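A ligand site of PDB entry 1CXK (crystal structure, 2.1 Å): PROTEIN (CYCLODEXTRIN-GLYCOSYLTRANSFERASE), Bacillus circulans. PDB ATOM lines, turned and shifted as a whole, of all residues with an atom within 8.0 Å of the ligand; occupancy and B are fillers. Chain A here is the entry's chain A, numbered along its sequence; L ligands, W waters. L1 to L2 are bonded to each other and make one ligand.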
ATOM      1  N   TYR A 301     -14.157  26.396  12.979  1.00  0.00           N
ATOM      2  CA  TYR A 301     -14.711  27.712  12.738  1.00  0.00           C
ATOM      3  C   TYR A 301     -15.944  27.971  13.594  1.00  0.00           C
ATOM      4  O   TYR A 301     -16.146  29.078  14.081  1.00  0.00           O
ATOM      5  CB  TYR A 301     -14.965  28.009  11.245  1.00  0.00           C
ATOM      6  CG  TYR A 301     -13.660  27.966  10.480  1.00  0.00           C
ATOM      7  CD1 TYR A 301     -12.765  29.032  10.531  1.00  0.00           C
ATOM      8  CD2 TYR A 301     -13.316  26.836   9.744  1.00  0.00           C
ATOM      9  CE1 TYR A 301     -11.549  28.988   9.843  1.00  0.00           C
ATOM     10  CE2 TYR A 301     -12.107  26.771   9.046  1.00  0.00           C
ATOM     11  CZ  TYR A 301     -11.225  27.855   9.108  1.00  0.00           C
ATOM     12  OH  TYR A 301     -10.046  27.789   8.418  1.00  0.00           O
ATOM     13  N   LYS A 304     -14.832  28.449  17.290  1.00  0.00           N
ATOM     14  CA  LYS A 304     -14.358  29.815  17.468  1.00  0.00           C
ATOM     15  C   LYS A 304     -15.507  30.817  17.522  1.00  0.00           C
ATOM     16  O   LYS A 304     -15.515  31.744  18.347  1.00  0.00           O
ATOM     17  CB  LYS A 304     -13.326  30.204  16.428  1.00  0.00           C
ATOM     18  CG  LYS A 304     -13.213  31.705  16.182  1.00  0.00           C
ATOM     19  CD  LYS A 304     -12.160  32.038  15.146  1.00  0.00           C
ATOM     20  CE  LYS A 304     -12.281  33.441  14.565  1.00  0.00           C
ATOM     21  NZ  LYS A 304     -11.040  34.205  14.665  1.00  0.00           N
ATOM     22  N   GLN A 410      -8.587  34.288  22.969  1.00  0.00           N
ATOM     23  CA  GLN A 410      -8.219  34.759  21.643  1.00  0.00           C
ATOM     24  C   GLN A 410      -7.690  33.654  20.729  1.00  0.00           C
ATOM     25  O   GLN A 410      -6.792  32.898  21.099  1.00  0.00           O
ATOM     26  CB  GLN A 410      -7.170  35.884  21.732  1.00  0.00           C
ATOM     27  CG  GLN A 410      -6.989  36.635  20.401  1.00  0.00           C
ATOM     28  CD  GLN A 410      -5.780  37.552  20.393  1.00  0.00           C
ATOM     29  OE1 GLN A 410      -5.059  37.676  21.395  1.00  0.00           O
ATOM     30  NE2 GLN A 410      -5.562  38.188  19.242  1.00  0.00           N
ATOM     31  N   GLU A 411      -8.267  33.548  19.535  1.00  0.00           N
ATOM     32  CA  GLU A 411      -7.832  32.552  18.572  1.00  0.00           C
ATOM     33  C   GLU A 411      -6.482  32.990  18.019  1.00  0.00           C
ATOM     34  O   GLU A 411      -6.288  34.164  17.726  1.00  0.00           O
ATOM     35  CB  GLU A 411      -8.878  32.351  17.453  1.00  0.00           C
ATOM     36  CG  GLU A 411      -8.345  31.559  16.241  1.00  0.00           C
ATOM     37  CD  GLU A 411      -7.827  32.440  15.137  1.00  0.00           C
ATOM     38  OE1 GLU A 411      -8.496  33.311  14.616  1.00  0.00           O
ATOM     39  OE2 GLU A 411      -6.583  32.184  14.827  1.00  0.00           O
ATOM     40  N   ARG A 412      -5.540  32.054  17.909  1.00  0.00           N
ATOM     41  CA  ARG A 412      -4.206  32.366  17.429  1.00  0.00           C
ATOM     42  C   ARG A 412      -3.826  31.622  16.155  1.00  0.00           C
ATOM     43  O   ARG A 412      -2.949  32.057  15.419  1.00  0.00           O
ATOM     44  CB  ARG A 412      -3.145  32.168  18.506  1.00  0.00           C
ATOM     45  CG  ARG A 412      -3.269  33.157  19.665  1.00  0.00           C
ATOM     46  CD  ARG A 412      -2.881  34.588  19.291  1.00  0.00           C
ATOM     47  NE  ARG A 412      -2.424  35.367  20.437  1.00  0.00           N
ATOM     48  CZ  ARG A 412      -1.853  36.570  20.372  1.00  0.00           C
ATOM     49  NH1 ARG A 412      -1.666  37.209  19.216  1.00  0.00           N
ATOM     50  NH2 ARG A 412      -1.474  37.164  21.491  1.00  0.00           N
ATOM     51  N   TRP A 413      -4.478  30.484  15.912  1.00  0.00           N
ATOM     52  CA  TRP A 413      -4.245  29.665  14.734  1.00  0.00           C
ATOM     53  C   TRP A 413      -5.501  28.855  14.432  1.00  0.00           C
ATOM     54  O   TRP A 413      -6.135  28.338  15.348  1.00  0.00           O
ATOM     55  CB  TRP A 413      -3.013  28.739  14.904  1.00  0.00           C
ATOM     56  CG  TRP A 413      -2.207  28.479  13.662  1.00  0.00           C
ATOM     57  CD1 TRP A 413      -1.103  29.155  13.273  1.00  0.00           C
ATOM     58  CD2 TRP A 413      -2.421  27.464  12.654  1.00  0.00           C
ATOM     59  NE1 TRP A 413      -0.604  28.648  12.105  1.00  0.00           N
ATOM     60  CE2 TRP A 413      -1.391  27.610  11.694  1.00  0.00           C
ATOM     61  CE3 TRP A 413      -3.374  26.469  12.475  1.00  0.00           C
ATOM     62  CZ2 TRP A 413      -1.297  26.782  10.579  1.00  0.00           C
ATOM     63  CZ3 TRP A 413      -3.292  25.653  11.364  1.00  0.00           C
ATOM     64  CH2 TRP A 413      -2.263  25.802  10.426  1.00  0.00           C
ATOM     65  N   ILE A 414      -5.889  28.762  13.165  1.00  0.00           N
ATOM     66  CA  ILE A 414      -7.093  28.002  12.884  1.00  0.00           C
ATOM     67  C   ILE A 414      -7.239  27.479  11.462  1.00  0.00           C
ATOM     68  O   ILE A 414      -6.829  28.091  10.482  1.00  0.00           O
ATOM     69  CB  ILE A 414      -8.325  28.788  13.307  1.00  0.00           C
ATOM     70  CG1 ILE A 414      -9.581  27.945  13.187  1.00  0.00           C
ATOM     71  CG2 ILE A 414      -8.485  30.046  12.445  1.00  0.00           C
ATOM     72  CD1 ILE A 414     -10.845  28.723  13.503  1.00  0.00           C
ATOM     73  N   ASN A 415      -7.872  26.316  11.373  1.00  0.00           N
ATOM     74  CA  ASN A 415      -8.220  25.649  10.124  1.00  0.00           C
ATOM     75  C   ASN A 415      -9.415  24.750  10.401  1.00  0.00           C
ATOM     76  O   ASN A 415      -9.988  24.835  11.483  1.00  0.00           O
ATOM     77  CB  ASN A 415      -7.063  24.998   9.333  1.00  0.00           C
ATOM     78  CG  ASN A 415      -6.563  23.686   9.894  1.00  0.00           C
ATOM     79  OD1 ASN A 415      -7.250  23.009  10.669  1.00  0.00           O
ATOM     80  ND2 ASN A 415      -5.367  23.297   9.463  1.00  0.00           N
ATOM     81  N   ASN A 416      -9.801  23.895   9.459  1.00  0.00           N
ATOM     82  CA  ASN A 416     -10.952  23.021   9.687  1.00  0.00           C
ATOM     83  C   ASN A 416     -10.828  22.155  10.923  1.00  0.00           C
ATOM     84  O   ASN A 416     -11.814  21.905  11.618  1.00  0.00           O
ATOM     85  CB  ASN A 416     -11.216  22.038   8.530  1.00  0.00           C
ATOM     86  CG  ASN A 416     -11.845  22.674   7.311  1.00  0.00           C
ATOM     87  OD1 ASN A 416     -11.926  22.067   6.245  1.00  0.00           O
ATOM     88  ND2 ASN A 416     -12.276  23.924   7.469  1.00  0.00           N
ATOM     89  N   VAL A 418      -7.864  22.318  13.200  1.00  0.00           N
ATOM     90  CA  VAL A 418      -7.034  22.838  14.273  1.00  0.00           C
ATOM     91  C   VAL A 418      -7.535  24.136  14.889  1.00  0.00           C
ATOM     92  O   VAL A 418      -7.992  25.054  14.213  1.00  0.00           O
ATOM     93  CB  VAL A 418      -5.611  23.066  13.786  1.00  0.00           C
ATOM     94  CG1 VAL A 418      -4.733  23.607  14.911  1.00  0.00           C
ATOM     95  CG2 VAL A 418      -5.001  21.787  13.218  1.00  0.00           C
ATOM     96  N   LEU A 419      -7.376  24.205  16.208  1.00  0.00           N
ATOM     97  CA  LEU A 419      -7.703  25.408  16.956  1.00  0.00           C
ATOM     98  C   LEU A 419      -6.618  25.663  17.982  1.00  0.00           C
ATOM     99  O   LEU A 419      -6.340  24.792  18.813  1.00  0.00           O
ATOM    100  CB  LEU A 419      -9.099  25.485  17.602  1.00  0.00           C
ATOM    101  CG  LEU A 419      -9.302  26.831  18.303  1.00  0.00           C
ATOM    102  CD1 LEU A 419      -9.239  27.973  17.300  1.00  0.00           C
ATOM    103  CD2 LEU A 419     -10.638  26.873  19.041  1.00  0.00           C
ATOM    104  N   ILE A 420      -6.011  26.836  17.917  1.00  0.00           N
ATOM    105  CA  ILE A 420      -4.985  27.230  18.877  1.00  0.00           C
ATOM    106  C   ILE A 420      -5.465  28.527  19.521  1.00  0.00           C
ATOM    107  O   ILE A 420      -5.605  29.546  18.860  1.00  0.00           O
ATOM    108  CB  ILE A 420      -3.590  27.372  18.277  1.00  0.00           C
ATOM    109  CG1 ILE A 420      -3.161  26.073  17.593  1.00  0.00           C
ATOM    110  CG2 ILE A 420      -2.583  27.717  19.366  1.00  0.00           C
ATOM    111  CD1 ILE A 420      -1.709  26.092  17.118  1.00  0.00           C
ATOM    112  N   SER A 443       0.755  21.099  10.060  1.00  0.00           N
ATOM    113  CA  SER A 443       2.011  21.823  10.080  1.00  0.00           C
ATOM    114  C   SER A 443       1.739  23.239  10.568  1.00  0.00           C
ATOM    115  O   SER A 443       1.092  24.032   9.896  1.00  0.00           O
ATOM    116  CB  SER A 443       2.706  21.760   8.729  1.00  0.00           C
ATOM    117  OG  SER A 443       3.955  22.423   8.789  1.00  0.00           O
ATOM    118  N   ILE A 444       2.217  23.543  11.774  1.00  0.00           N
ATOM    119  CA  ILE A 444       1.968  24.851  12.349  1.00  0.00           C
ATOM    120  C   ILE A 444       3.093  25.869  12.227  1.00  0.00           C
ATOM    121  O   ILE A 444       4.135  25.770  12.870  1.00  0.00           O
ATOM    122  CB  ILE A 444       1.336  24.749  13.747  1.00  0.00           C
ATOM    123  CG1 ILE A 444      -0.077  24.191  13.585  1.00  0.00           C
ATOM    124  CG2 ILE A 444       1.262  26.110  14.415  1.00  0.00           C
ATOM    125  CD1 ILE A 444      -0.292  22.914  14.372  1.00  0.00           C
ATOM    126  N   SER A 445       2.841  26.864  11.388  1.00  0.00           N
ATOM    127  CA  SER A 445       3.777  27.953  11.160  1.00  0.00           C
ATOM    128  C   SER A 445       3.015  29.270  11.212  1.00  0.00           C
ATOM    129  O   SER A 445       1.830  29.302  10.903  1.00  0.00           O
ATOM    130  CB  SER A 445       4.602  27.806   9.879  1.00  0.00           C
ATOM    131  OG  SER A 445       3.783  27.742   8.728  1.00  0.00           O
ATOM    132  N   GLY A 446       3.696  30.330  11.633  1.00  0.00           N
ATOM    133  CA  GLY A 446       3.097  31.654  11.734  1.00  0.00           C
ATOM    134  C   GLY A 446       2.363  31.915  13.044  1.00  0.00           C
ATOM    135  O   GLY A 446       1.739  32.950  13.219  1.00  0.00           O
ATOM    136  N   LEU A 447       2.423  30.975  13.983  1.00  0.00           N
ATOM    137  CA  LEU A 447       1.751  31.174  15.257  1.00  0.00           C
ATOM    138  C   LEU A 447       2.389  32.293  16.058  1.00  0.00           C
ATOM    139  O   LEU A 447       3.609  32.323  16.231  1.00  0.00           O
ATOM    140  CB  LEU A 447       1.684  29.878  16.097  1.00  0.00           C
ATOM    141  CG  LEU A 447       1.217  30.091  17.541  1.00  0.00           C
ATOM    142  CD1 LEU A 447      -0.280  30.362  17.595  1.00  0.00           C
ATOM    143  CD2 LEU A 447       1.535  28.858  18.392  1.00  0.00           C
ATOM    144  N   VAL A 448       1.563  33.201  16.552  1.00  0.00           N
ATOM    145  CA  VAL A 448       2.008  34.318  17.370  1.00  0.00           C
ATOM    146  C   VAL A 448       1.236  34.300  18.684  1.00  0.00           C
ATOM    147  O   VAL A 448       0.023  34.091  18.694  1.00  0.00           O
ATOM    148  CB  VAL A 448       1.834  35.666  16.675  1.00  0.00           C
ATOM    149  CG1 VAL A 448       1.976  36.791  17.685  1.00  0.00           C
ATOM    150  CG2 VAL A 448       2.887  35.834  15.581  1.00  0.00           C
ATOM    151  N   THR A 449       1.933  34.515  19.804  1.00  0.00           N
ATOM    152  CA  THR A 449       1.310  34.518  21.119  1.00  0.00           C
ATOM    153  C   THR A 449       1.851  35.623  22.017  1.00  0.00           C
ATOM    154  O   THR A 449       2.722  36.395  21.622  1.00  0.00           O
ATOM    155  CB  THR A 449       1.514  33.176  21.850  1.00  0.00           C
ATOM    156  OG1 THR A 449       2.839  33.124  22.334  1.00  0.00           O
ATOM    157  CG2 THR A 449       1.291  32.002  20.901  1.00  0.00           C
ATOM    158  N   ALA A 476       6.550  35.062  18.718  1.00  0.00           N
ATOM    159  CA  ALA A 476       6.449  34.182  17.570  1.00  0.00           C
ATOM    160  C   ALA A 476       6.980  32.786  17.862  1.00  0.00           C
ATOM    161  O   ALA A 476       8.122  32.615  18.285  1.00  0.00           O
ATOM    162  CB  ALA A 476       7.161  34.789  16.371  1.00  0.00           C
HETATM  163  C1  LIG L   1      -2.479  29.613   8.606  1.00  0.00           C
HETATM  164  C2  LIG L   1      -3.591  29.473   9.601  1.00  0.00           C
HETATM  165  C3  LIG L   1      -3.969  30.820  10.197  1.00  0.00           C
HETATM  166  C4  LIG L   1      -2.723  31.502  10.743  1.00  0.00           C
HETATM  167  C5  LIG L   1      -1.649  31.618   9.674  1.00  0.00           C
HETATM  168  C6  LIG L   1      -0.339  32.126  10.236  1.00  0.00           C
HETATM  169  O1  LIG L   1      -2.899  30.227   7.436  1.00  0.00           O
HETATM  170  O2  LIG L   1      -4.729  28.862   8.982  1.00  0.00           O
HETATM  171  O3  LIG L   1      -4.927  30.623  11.223  1.00  0.00           O
HETATM  172  O4  LIG L   1      -3.090  32.825  11.198  1.00  0.00           O
HETATM  173  O5  LIG L   1      -1.382  30.284   9.216  1.00  0.00           O
HETATM  174  O6  LIG L   1       0.594  32.289   9.169  1.00  0.00           O
HETATM  175  C1  LG2 L   2      -2.975  33.127  12.560  1.00  0.00           C
HETATM  176  C2  LG2 L   2      -4.236  33.854  12.996  1.00  0.00           C
HETATM  177  C3  LG2 L   2      -4.297  35.201  12.338  1.00  0.00           C
HETATM  178  C4  LG2 L   2      -3.029  35.999  12.601  1.00  0.00           C
HETATM  179  C5  LG2 L   2      -1.803  35.192  12.203  1.00  0.00           C
HETATM  180  C6  LG2 L   2      -0.560  35.884  12.693  1.00  0.00           C
HETATM  181  O1  LG2 L   2      -5.359  33.079  12.600  1.00  0.00           O
HETATM  182  O2  LG2 L   2      -5.373  35.982  12.867  1.00  0.00           O
HETATM  183  O3  LG2 L   2      -2.999  37.172  11.792  1.00  0.00           O
HETATM  184  O4  LG2 L   2      -1.814  33.898  12.817  1.00  0.00           O
HETATM  185  O5  LG2 L   2       0.613  35.380  12.070  1.00  0.00           O
HETATM  186  O   HOH W   1      -0.893  33.814  15.454  1.00  0.00           O
HETATM  187  O   HOH W   2      -8.055  29.583   8.614  1.00  0.00           O
HETATM  188  O   HOH W   3      -4.770  36.114  15.869  1.00  0.00           O
HETATM  189  O   HOH W   4       1.090  29.781   8.369  1.00  0.00           O
HETATM  190  O   HOH W   5      -8.149  34.641  12.033  1.00  0.00           O
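The backbone NH of Ile 414 lies within hydrogen-bond range of an oxygen (O3) of LIG L1 (2.9 Å).
O of Ile 414 is in hydrogen-bond range of O2 of LIG L1.
The side-chain carboxylate (OE2) of Glu 411 is in hydrogen-bond range of an oxygen (O1) of LG2 L2, 2.7 Å away.
The backbone carbonyl oxygen (O) of Gly 446 sits at hydrogen-bond distance from an oxygen (O5) of LG2 L2.
O5 of LIG L1 is in hydrogen-bond range of NE1 of Trp 413 (3.4 Å).
N of Trp 413 sits at hydrogen-bond distance from OE2 of Glu 411, 2.9 Å away.
The side-chain amino group (NZ) of Lys 304 is in salt-bridge range of the side-chain carboxylate (OE1) of Glu 411, at 2.7 Å.
The backbone carbonyl oxygen (O) of Val 448 sits close to the guanidinium group (NE) of Arg 412, 3.3 Å away.
The backbone NH (N) of Arg 412 lies within hydrogen-bond range of the backbone carbonyl oxygen (O) of Ile 420 (2.7 Å).
NE1 of Trp 413 lies within hydrogen-bond range of O of Ser 445, at 2.8 Å.
The backbone carbonyl oxygen of Trp 413 lies within hydrogen-bond range of the backbone NH of Ile 420 (3.0 Å).
O of Arg 412 sits close to O4 of LG2 L2 (3.4 Å).
O of Ser 445 touches C6 of LIG L1 (3.6 Å).
Six residues have an atom within 4 Å of the ligand: Glu 411, Arg 412, Trp 413, Ile 414, Ser 445 and Gly 446.
The nearest printed residue that does not touch the ligand is Val 448 (4.2 Å).
Water W4 lies within hydrogen-bond range of O5 of LIG L1 (2.7 Å) and O of Ser 445 (2.7 Å).
Water W1 lies within hydrogen-bond range of O of Arg 412, N of Val 448 and O4 of LG2 L2.
Water W3 lies within hydrogen-bond range of an oxygen (O2) of LG2 L2 (3.1 Å) and the backbone carbonyl oxygen of Glu 411 (3.1 Å).
Water W5 bridges OE1 of Glu 411 (2.9 Å) and O2 of LG2 L2 (3.2 Å).
Water W2 lies within hydrogen-bond range of O of Ile 414 (2.7 Å), OH of Tyr 301 (2.7 Å) and O2 of LIG L1 (3.4 Å).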
